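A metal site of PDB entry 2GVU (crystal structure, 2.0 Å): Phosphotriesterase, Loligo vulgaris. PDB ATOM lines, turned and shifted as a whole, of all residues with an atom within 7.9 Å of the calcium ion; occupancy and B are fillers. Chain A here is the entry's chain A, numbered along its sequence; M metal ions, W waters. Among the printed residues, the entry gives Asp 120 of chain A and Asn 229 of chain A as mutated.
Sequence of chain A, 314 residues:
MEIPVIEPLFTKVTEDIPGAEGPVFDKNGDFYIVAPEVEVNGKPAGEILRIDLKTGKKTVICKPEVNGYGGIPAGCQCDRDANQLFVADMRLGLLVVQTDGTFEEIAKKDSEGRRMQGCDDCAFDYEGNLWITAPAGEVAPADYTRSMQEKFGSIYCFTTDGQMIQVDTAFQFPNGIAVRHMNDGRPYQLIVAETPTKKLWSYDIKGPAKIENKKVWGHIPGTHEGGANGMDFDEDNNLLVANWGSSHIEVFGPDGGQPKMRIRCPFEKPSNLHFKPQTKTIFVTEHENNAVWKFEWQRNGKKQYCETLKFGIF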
ATOM      1  N   ALA A  20       5.288  -5.967 -22.131  1.00  0.00           N
ATOM      2  CA  ALA A  20       5.859  -4.670 -21.784  1.00  0.00           C
ATOM      3  C   ALA A  20       6.672  -4.711 -20.496  1.00  0.00           C
ATOM      4  O   ALA A  20       6.146  -5.038 -19.425  1.00  0.00           O
ATOM      5  CB  ALA A  20       4.746  -3.630 -21.661  1.00  0.00           C
ATOM      6  N   GLU A  21       7.954  -4.379 -20.589  1.00  0.00           N
ATOM      7  CA  GLU A  21       8.854  -4.417 -19.450  1.00  0.00           C
ATOM      8  C   GLU A  21       9.993  -3.399 -19.572  1.00  0.00           C
ATOM      9  O   GLU A  21      10.056  -2.638 -20.544  1.00  0.00           O
ATOM     10  CB  GLU A  21       9.455  -5.829 -19.326  1.00  0.00           C
ATOM     11  CG  GLU A  21       8.881  -6.678 -18.196  1.00  0.00           C
ATOM     12  CD  GLU A  21       9.600  -6.458 -16.877  1.00  0.00           C
ATOM     13  OE1 GLU A  21      10.128  -5.353 -16.661  1.00  0.00           O
ATOM     14  OE2 GLU A  21       9.613  -7.392 -16.042  1.00  0.00           O
ATOM     15  N   GLY A  22      10.865  -3.409 -18.571  1.00  0.00           N
ATOM     16  CA  GLY A  22      12.040  -2.543 -18.547  1.00  0.00           C
ATOM     17  C   GLY A  22      11.950  -1.068 -18.911  1.00  0.00           C
ATOM     18  O   GLY A  22      12.752  -0.593 -19.721  1.00  0.00           O
ATOM     19  N   ALA A  74      14.253  -7.977 -21.126  1.00  0.00           N
ATOM     20  CA  ALA A  74      13.299  -7.758 -20.055  1.00  0.00           C
ATOM     21  C   ALA A  74      13.572  -6.616 -19.090  1.00  0.00           C
ATOM     22  O   ALA A  74      12.637  -6.121 -18.452  1.00  0.00           O
ATOM     23  CB  ALA A  74      13.150  -9.048 -19.260  1.00  0.00           C
ATOM     24  N   GLY A  75      14.824  -6.187 -18.957  1.00  0.00           N
ATOM     25  CA  GLY A  75      15.133  -5.110 -18.026  1.00  0.00           C
ATOM     26  C   GLY A  75      16.241  -4.207 -18.529  1.00  0.00           C
ATOM     27  O   GLY A  75      17.129  -4.669 -19.239  1.00  0.00           O
ATOM     28  N   MET A  90      16.583 -12.518 -21.137  1.00  0.00           N
ATOM     29  CA  MET A  90      16.369 -13.875 -20.640  1.00  0.00           C
ATOM     30  C   MET A  90      17.040 -14.935 -21.497  1.00  0.00           C
ATOM     31  O   MET A  90      17.316 -16.026 -21.009  1.00  0.00           O
ATOM     32  CB  MET A  90      14.876 -14.169 -20.519  1.00  0.00           C
ATOM     33  CG  MET A  90      14.168 -13.401 -19.406  1.00  0.00           C
ATOM     34  SD  MET A  90      14.591 -13.994 -17.745  1.00  0.00           S
ATOM     35  CE  MET A  90      13.401 -15.351 -17.604  1.00  0.00           C
ATOM     36  N   CYS A 119      19.162 -13.276 -18.041  1.00  0.00           N
ATOM     37  CA  CYS A 119      18.889 -12.222 -17.066  1.00  0.00           C
ATOM     38  C   CYS A 119      17.526 -11.545 -17.185  1.00  0.00           C
ATOM     39  O   CYS A 119      16.916 -11.533 -18.253  1.00  0.00           O
ATOM     40  CB  CYS A 119      19.998 -11.176 -17.136  1.00  0.00           C
ATOM     41  SG  CYS A 119      21.606 -11.890 -16.748  1.00  0.00           S
ATOM     42  N   ASP A 120      17.062 -10.957 -16.086  1.00  0.00           N
ATOM     43  CA  ASP A 120      15.763 -10.312 -16.058  1.00  0.00           C
ATOM     44  C   ASP A 120      15.799  -8.788 -15.823  1.00  0.00           C
ATOM     45  O   ASP A 120      15.214  -8.042 -16.599  1.00  0.00           O
ATOM     46  CB  ASP A 120      14.899 -10.985 -14.989  1.00  0.00           C
ATOM     47  CG  ASP A 120      13.441 -10.544 -15.041  1.00  0.00           C
ATOM     48  OD1 ASP A 120      13.153  -9.363 -14.806  1.00  0.00           O
ATOM     49  OD2 ASP A 120      12.582 -11.407 -15.313  1.00  0.00           O
ATOM     50  N   ASP A 121      16.466  -8.338 -14.771  1.00  0.00           N
ATOM     51  CA  ASP A 121      16.531  -6.904 -14.484  1.00  0.00           C
ATOM     52  C   ASP A 121      17.909  -6.570 -13.931  1.00  0.00           C
ATOM     53  O   ASP A 121      18.682  -7.464 -13.593  1.00  0.00           O
ATOM     54  CB  ASP A 121      15.454  -6.518 -13.458  1.00  0.00           C
ATOM     55  CG  ASP A 121      14.887  -5.110 -13.679  1.00  0.00           C
ATOM     56  OD1 ASP A 121      15.540  -4.276 -14.338  1.00  0.00           O
ATOM     57  OD2 ASP A 121      13.784  -4.834 -13.170  1.00  0.00           O
ATOM     58  N   CYS A 122      18.221  -5.282 -13.837  1.00  0.00           N
ATOM     59  CA  CYS A 122      19.521  -4.861 -13.337  1.00  0.00           C
ATOM     60  C   CYS A 122      19.433  -3.476 -12.704  1.00  0.00           C
ATOM     61  O   CYS A 122      18.477  -2.745 -12.927  1.00  0.00           O
ATOM     62  CB  CYS A 122      20.543  -4.847 -14.485  1.00  0.00           C
ATOM     63  SG  CYS A 122      19.980  -3.954 -15.952  1.00  0.00           S
ATOM     64  N   THR A 133      19.807  -9.702 -11.893  1.00  0.00           N
ATOM     65  CA  THR A 133      19.098 -10.899 -11.469  1.00  0.00           C
ATOM     66  C   THR A 133      19.014 -11.839 -12.674  1.00  0.00           C
ATOM     67  O   THR A 133      18.818 -11.408 -13.812  1.00  0.00           O
ATOM     68  CB  THR A 133      17.665 -10.591 -10.965  1.00  0.00           C
ATOM     69  OG1 THR A 133      16.935  -9.920 -11.998  1.00  0.00           O
ATOM     70  CG2 THR A 133      17.719  -9.735  -9.715  1.00  0.00           C
ATOM     71  N   PRO A 135      16.963 -15.192 -13.464  1.00  0.00           N
ATOM     72  CA  PRO A 135      15.963 -16.221 -13.188  1.00  0.00           C
ATOM     73  C   PRO A 135      15.916 -17.364 -14.211  1.00  0.00           C
ATOM     74  O   PRO A 135      15.362 -18.426 -13.944  1.00  0.00           O
ATOM     75  CB  PRO A 135      14.671 -15.432 -13.151  1.00  0.00           C
ATOM     76  CG  PRO A 135      14.896 -14.426 -14.240  1.00  0.00           C
ATOM     77  CD  PRO A 135      16.336 -13.982 -14.021  1.00  0.00           C
ATOM     78  N   PHE A 173      13.306 -17.702  -9.044  1.00  0.00           N
ATOM     79  CA  PHE A 173      12.977 -16.574  -9.900  1.00  0.00           C
ATOM     80  C   PHE A 173      13.288 -15.184  -9.324  1.00  0.00           C
ATOM     81  O   PHE A 173      12.391 -14.442  -8.928  1.00  0.00           O
ATOM     82  CB  PHE A 173      11.505 -16.634 -10.354  1.00  0.00           C
ATOM     83  CG  PHE A 173      11.269 -16.045 -11.722  1.00  0.00           C
ATOM     84  CD1 PHE A 173      11.246 -14.662 -11.918  1.00  0.00           C
ATOM     85  CD2 PHE A 173      11.154 -16.876 -12.844  1.00  0.00           C
ATOM     86  CE1 PHE A 173      11.120 -14.110 -13.185  1.00  0.00           C
ATOM     87  CE2 PHE A 173      11.039 -16.339 -14.127  1.00  0.00           C
ATOM     88  CZ  PHE A 173      11.022 -14.954 -14.302  1.00  0.00           C
ATOM     89  N   PRO A 174      14.586 -14.835  -9.242  1.00  0.00           N
ATOM     90  CA  PRO A 174      14.958 -13.522  -8.716  1.00  0.00           C
ATOM     91  C   PRO A 174      14.494 -12.566  -9.833  1.00  0.00           C
ATOM     92  O   PRO A 174      14.690 -12.858 -11.013  1.00  0.00           O
ATOM     93  CB  PRO A 174      16.474 -13.606  -8.601  1.00  0.00           C
ATOM     94  CG  PRO A 174      16.845 -14.574  -9.696  1.00  0.00           C
ATOM     95  CD  PRO A 174      15.773 -15.637  -9.579  1.00  0.00           C
ATOM     96  N   ASN A 175      13.887 -11.446  -9.466  1.00  0.00           N
ATOM     97  CA  ASN A 175      13.334 -10.541 -10.472  1.00  0.00           C
ATOM     98  C   ASN A 175      13.816  -9.092 -10.346  1.00  0.00           C
ATOM     99  O   ASN A 175      14.869  -8.725 -10.880  1.00  0.00           O
ATOM    100  CB  ASN A 175      11.802 -10.588 -10.358  1.00  0.00           C
ATOM    101  CG  ASN A 175      11.118 -10.278 -11.659  1.00  0.00           C
ATOM    102  OD1 ASN A 175      11.568  -9.440 -12.430  1.00  0.00           O
ATOM    103  ND2 ASN A 175       9.987 -10.935 -11.896  1.00  0.00           N
ATOM    104  N   GLY A 176      13.020  -8.276  -9.670  1.00  0.00           N
ATOM    105  CA  GLY A 176      13.380  -6.890  -9.480  1.00  0.00           C
ATOM    106  C   GLY A 176      14.614  -6.797  -8.596  1.00  0.00           C
ATOM    107  O   GLY A 176      14.887  -7.688  -7.792  1.00  0.00           O
ATOM    108  N   ILE A 177      15.358  -5.709  -8.740  1.00  0.00           N
ATOM    109  CA  ILE A 177      16.563  -5.513  -7.947  1.00  0.00           C
ATOM    110  C   ILE A 177      16.805  -4.017  -7.832  1.00  0.00           C
ATOM    111  O   ILE A 177      16.573  -3.258  -8.778  1.00  0.00           O
ATOM    112  CB  ILE A 177      17.758  -6.232  -8.616  1.00  0.00           C
ATOM    113  CG1 ILE A 177      19.006  -6.092  -7.747  1.00  0.00           C
ATOM    114  CG2 ILE A 177      17.971  -5.680 -10.026  1.00  0.00           C
ATOM    115  CD1 ILE A 177      20.141  -7.020  -8.171  1.00  0.00           C
ATOM    116  N   THR A 195      10.065 -13.425  -6.871  1.00  0.00           N
ATOM    117  CA  THR A 195       8.659 -13.432  -7.243  1.00  0.00           C
ATOM    118  C   THR A 195       7.650 -14.397  -6.616  1.00  0.00           C
ATOM    119  O   THR A 195       6.830 -13.983  -5.796  1.00  0.00           O
ATOM    120  CB  THR A 195       8.535 -13.500  -8.784  1.00  0.00           C
ATOM    121  OG1 THR A 195       9.339 -12.455  -9.370  1.00  0.00           O
ATOM    122  CG2 THR A 195       7.083 -13.289  -9.216  1.00  0.00           C
ATOM    123  N   ALA A 228       6.309  -9.838  -6.401  1.00  0.00           N
ATOM    124  CA  ALA A 228       7.183  -8.728  -6.763  1.00  0.00           C
ATOM    125  C   ALA A 228       7.878  -8.912  -8.104  1.00  0.00           C
ATOM    126  O   ALA A 228       8.453  -9.963  -8.382  1.00  0.00           O
ATOM    127  CB  ALA A 228       8.231  -8.510  -5.673  1.00  0.00           C
ATOM    128  N   ASN A 229       7.799  -7.889  -8.948  1.00  0.00           N
ATOM    129  CA  ASN A 229       8.464  -7.929 -10.237  1.00  0.00           C
ATOM    130  C   ASN A 229       9.499  -6.796 -10.189  1.00  0.00           C
ATOM    131  O   ASN A 229      10.509  -6.908  -9.503  1.00  0.00           O
ATOM    132  CB  ASN A 229       7.461  -7.728 -11.380  1.00  0.00           C
ATOM    133  CG  ASN A 229       8.032  -8.166 -12.725  1.00  0.00           C
ATOM    134  OD1 ASN A 229       9.215  -7.982 -12.997  1.00  0.00           O
ATOM    135  ND2 ASN A 229       7.191  -8.741 -13.574  1.00  0.00           N
ATOM    136  N   GLY A 230       9.228  -5.680 -10.870  1.00  0.00           N
ATOM    137  CA  GLY A 230      10.169  -4.561 -10.880  1.00  0.00           C
ATOM    138  C   GLY A 230      10.077  -3.601  -9.707  1.00  0.00           C
ATOM    139  O   GLY A 230       9.024  -3.509  -9.063  1.00  0.00           O
ATOM    140  N   MET A 231      11.155  -2.862  -9.451  1.00  0.00           N
ATOM    141  CA  MET A 231      11.198  -1.914  -8.338  1.00  0.00           C
ATOM    142  C   MET A 231      12.143  -0.722  -8.566  1.00  0.00           C
ATOM    143  O   MET A 231      13.009  -0.755  -9.441  1.00  0.00           O
ATOM    144  CB  MET A 231      11.644  -2.632  -7.062  1.00  0.00           C
ATOM    145  CG  MET A 231      13.084  -3.172  -7.130  1.00  0.00           C
ATOM    146  SD  MET A 231      13.638  -4.131  -5.676  1.00  0.00           S
ATOM    147  CE  MET A 231      12.249  -5.152  -5.433  1.00  0.00           C
ATOM    148  N   SER A 271       4.173  -4.759 -14.069  1.00  0.00           N
ATOM    149  CA  SER A 271       5.404  -5.512 -14.199  1.00  0.00           C
ATOM    150  C   SER A 271       6.668  -4.769 -13.784  1.00  0.00           C
ATOM    151  O   SER A 271       7.547  -5.354 -13.158  1.00  0.00           O
ATOM    152  CB  SER A 271       5.557  -5.996 -15.659  1.00  0.00           C
ATOM    153  OG  SER A 271       5.691  -4.902 -16.556  1.00  0.00           O
ATOM    154  N   ASN A 272       6.768  -3.498 -14.129  1.00  0.00           N
ATOM    155  CA  ASN A 272       7.967  -2.736 -13.782  1.00  0.00           C
ATOM    156  C   ASN A 272       7.620  -1.255 -13.779  1.00  0.00           C
ATOM    157  O   ASN A 272       6.528  -0.866 -14.174  1.00  0.00           O
ATOM    158  CB  ASN A 272       9.092  -2.994 -14.795  1.00  0.00           C
ATOM    159  CG  ASN A 272      10.475  -3.012 -14.155  1.00  0.00           C
ATOM    160  OD1 ASN A 272      10.754  -2.276 -13.207  1.00  0.00           O
ATOM    161  ND2 ASN A 272      11.354  -3.853 -14.670  1.00  0.00           N
ATOM    162  N   THR A 285       4.828  -0.289 -16.595  1.00  0.00           N
ATOM    163  CA  THR A 285       4.531  -1.242 -17.652  1.00  0.00           C
ATOM    164  C   THR A 285       3.647  -2.302 -17.007  1.00  0.00           C
ATOM    165  O   THR A 285       3.802  -2.605 -15.822  1.00  0.00           O
ATOM    166  CB  THR A 285       5.824  -1.902 -18.217  1.00  0.00           C
ATOM    167  OG1 THR A 285       6.627  -2.396 -17.143  1.00  0.00           O
ATOM    168  CG2 THR A 285       6.647  -0.891 -19.038  1.00  0.00           C
ATOM    169  N   HIS A 287       1.184  -6.149 -17.776  1.00  0.00           N
ATOM    170  CA  HIS A 287       0.851  -7.268 -18.647  1.00  0.00           C
ATOM    171  C   HIS A 287      -0.613  -7.632 -18.827  1.00  0.00           C
ATOM    172  O   HIS A 287      -0.917  -8.671 -19.437  1.00  0.00           O
ATOM    173  CB  HIS A 287       1.629  -8.494 -18.173  1.00  0.00           C
ATOM    174  CG  HIS A 287       3.112  -8.320 -18.220  1.00  0.00           C
ATOM    175  ND1 HIS A 287       3.989  -9.160 -17.589  1.00  0.00           N
ATOM    176  CD2 HIS A 287       3.866  -7.379 -18.842  1.00  0.00           C
ATOM    177  CE1 HIS A 287       5.222  -8.759 -17.817  1.00  0.00           C
ATOM    178  NE2 HIS A 287       5.186  -7.681 -18.578  1.00  0.00           N
HETATM  179 CA    CA M   1      11.124  -8.233 -14.423  1.00  0.00          CA
HETATM  180  O   HOH W   1      10.215 -10.385 -14.995  1.00  0.00           O
HETATM  181  O   HOH W   2      12.054  -6.803 -12.729  1.00  0.00           O
HETATM  182  O   HOH W   3      12.678  -6.828 -15.785  1.00  0.00           O
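The backbone carbonyl oxygen of Asp 120 is in hydrogen-bond range of the backbone NH of Gly 75 (3.0 Å).
N of Asp 120 sits at hydrogen-bond distance from O of Thr 133, at 2.9 Å.
OE1 of Glu 21 lies within hydrogen-bond range of ND2 of Asn 272 (2.8 Å).
The side-chain hydroxyl (OG1) of Thr 133 sits at hydrogen-bond distance from the backbone carbonyl oxygen (O) of Asn 175 (2.6 Å).
The side-chain amide nitrogen of Asn 175 is in hydrogen-bond range of the side-chain hydroxyl of Thr 195.
The side-chain amide nitrogen of Asn 229 lies close to the backbone carbonyl oxygen of Ser 271, 3.4 Å away.
O of Asn 229 lies within hydrogen-bond range of N of Gly 176, 2.9 Å away.
Four residues have an atom within 4 Å of the calcium ion: Glu 21, Asp 120, Asn 175 and Asn 229.
The calcium ion is bound by the side-chain carboxylate of Asp 120 (2.4 Å), the side-chain carboxylate of Glu 21 (2.4 Å), the side-chain amide oxygen of Asn 175 (2.4 Å), the side-chain amide oxygen of Asn 229 (2.4 Å), water W1 (2.4 Å), water W2 (2.4 Å) and water W3 (2.5 Å).
Water W1 bridges the side-chain carboxylate of Asp 120 and the side-chain amide nitrogen of Asn 175.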
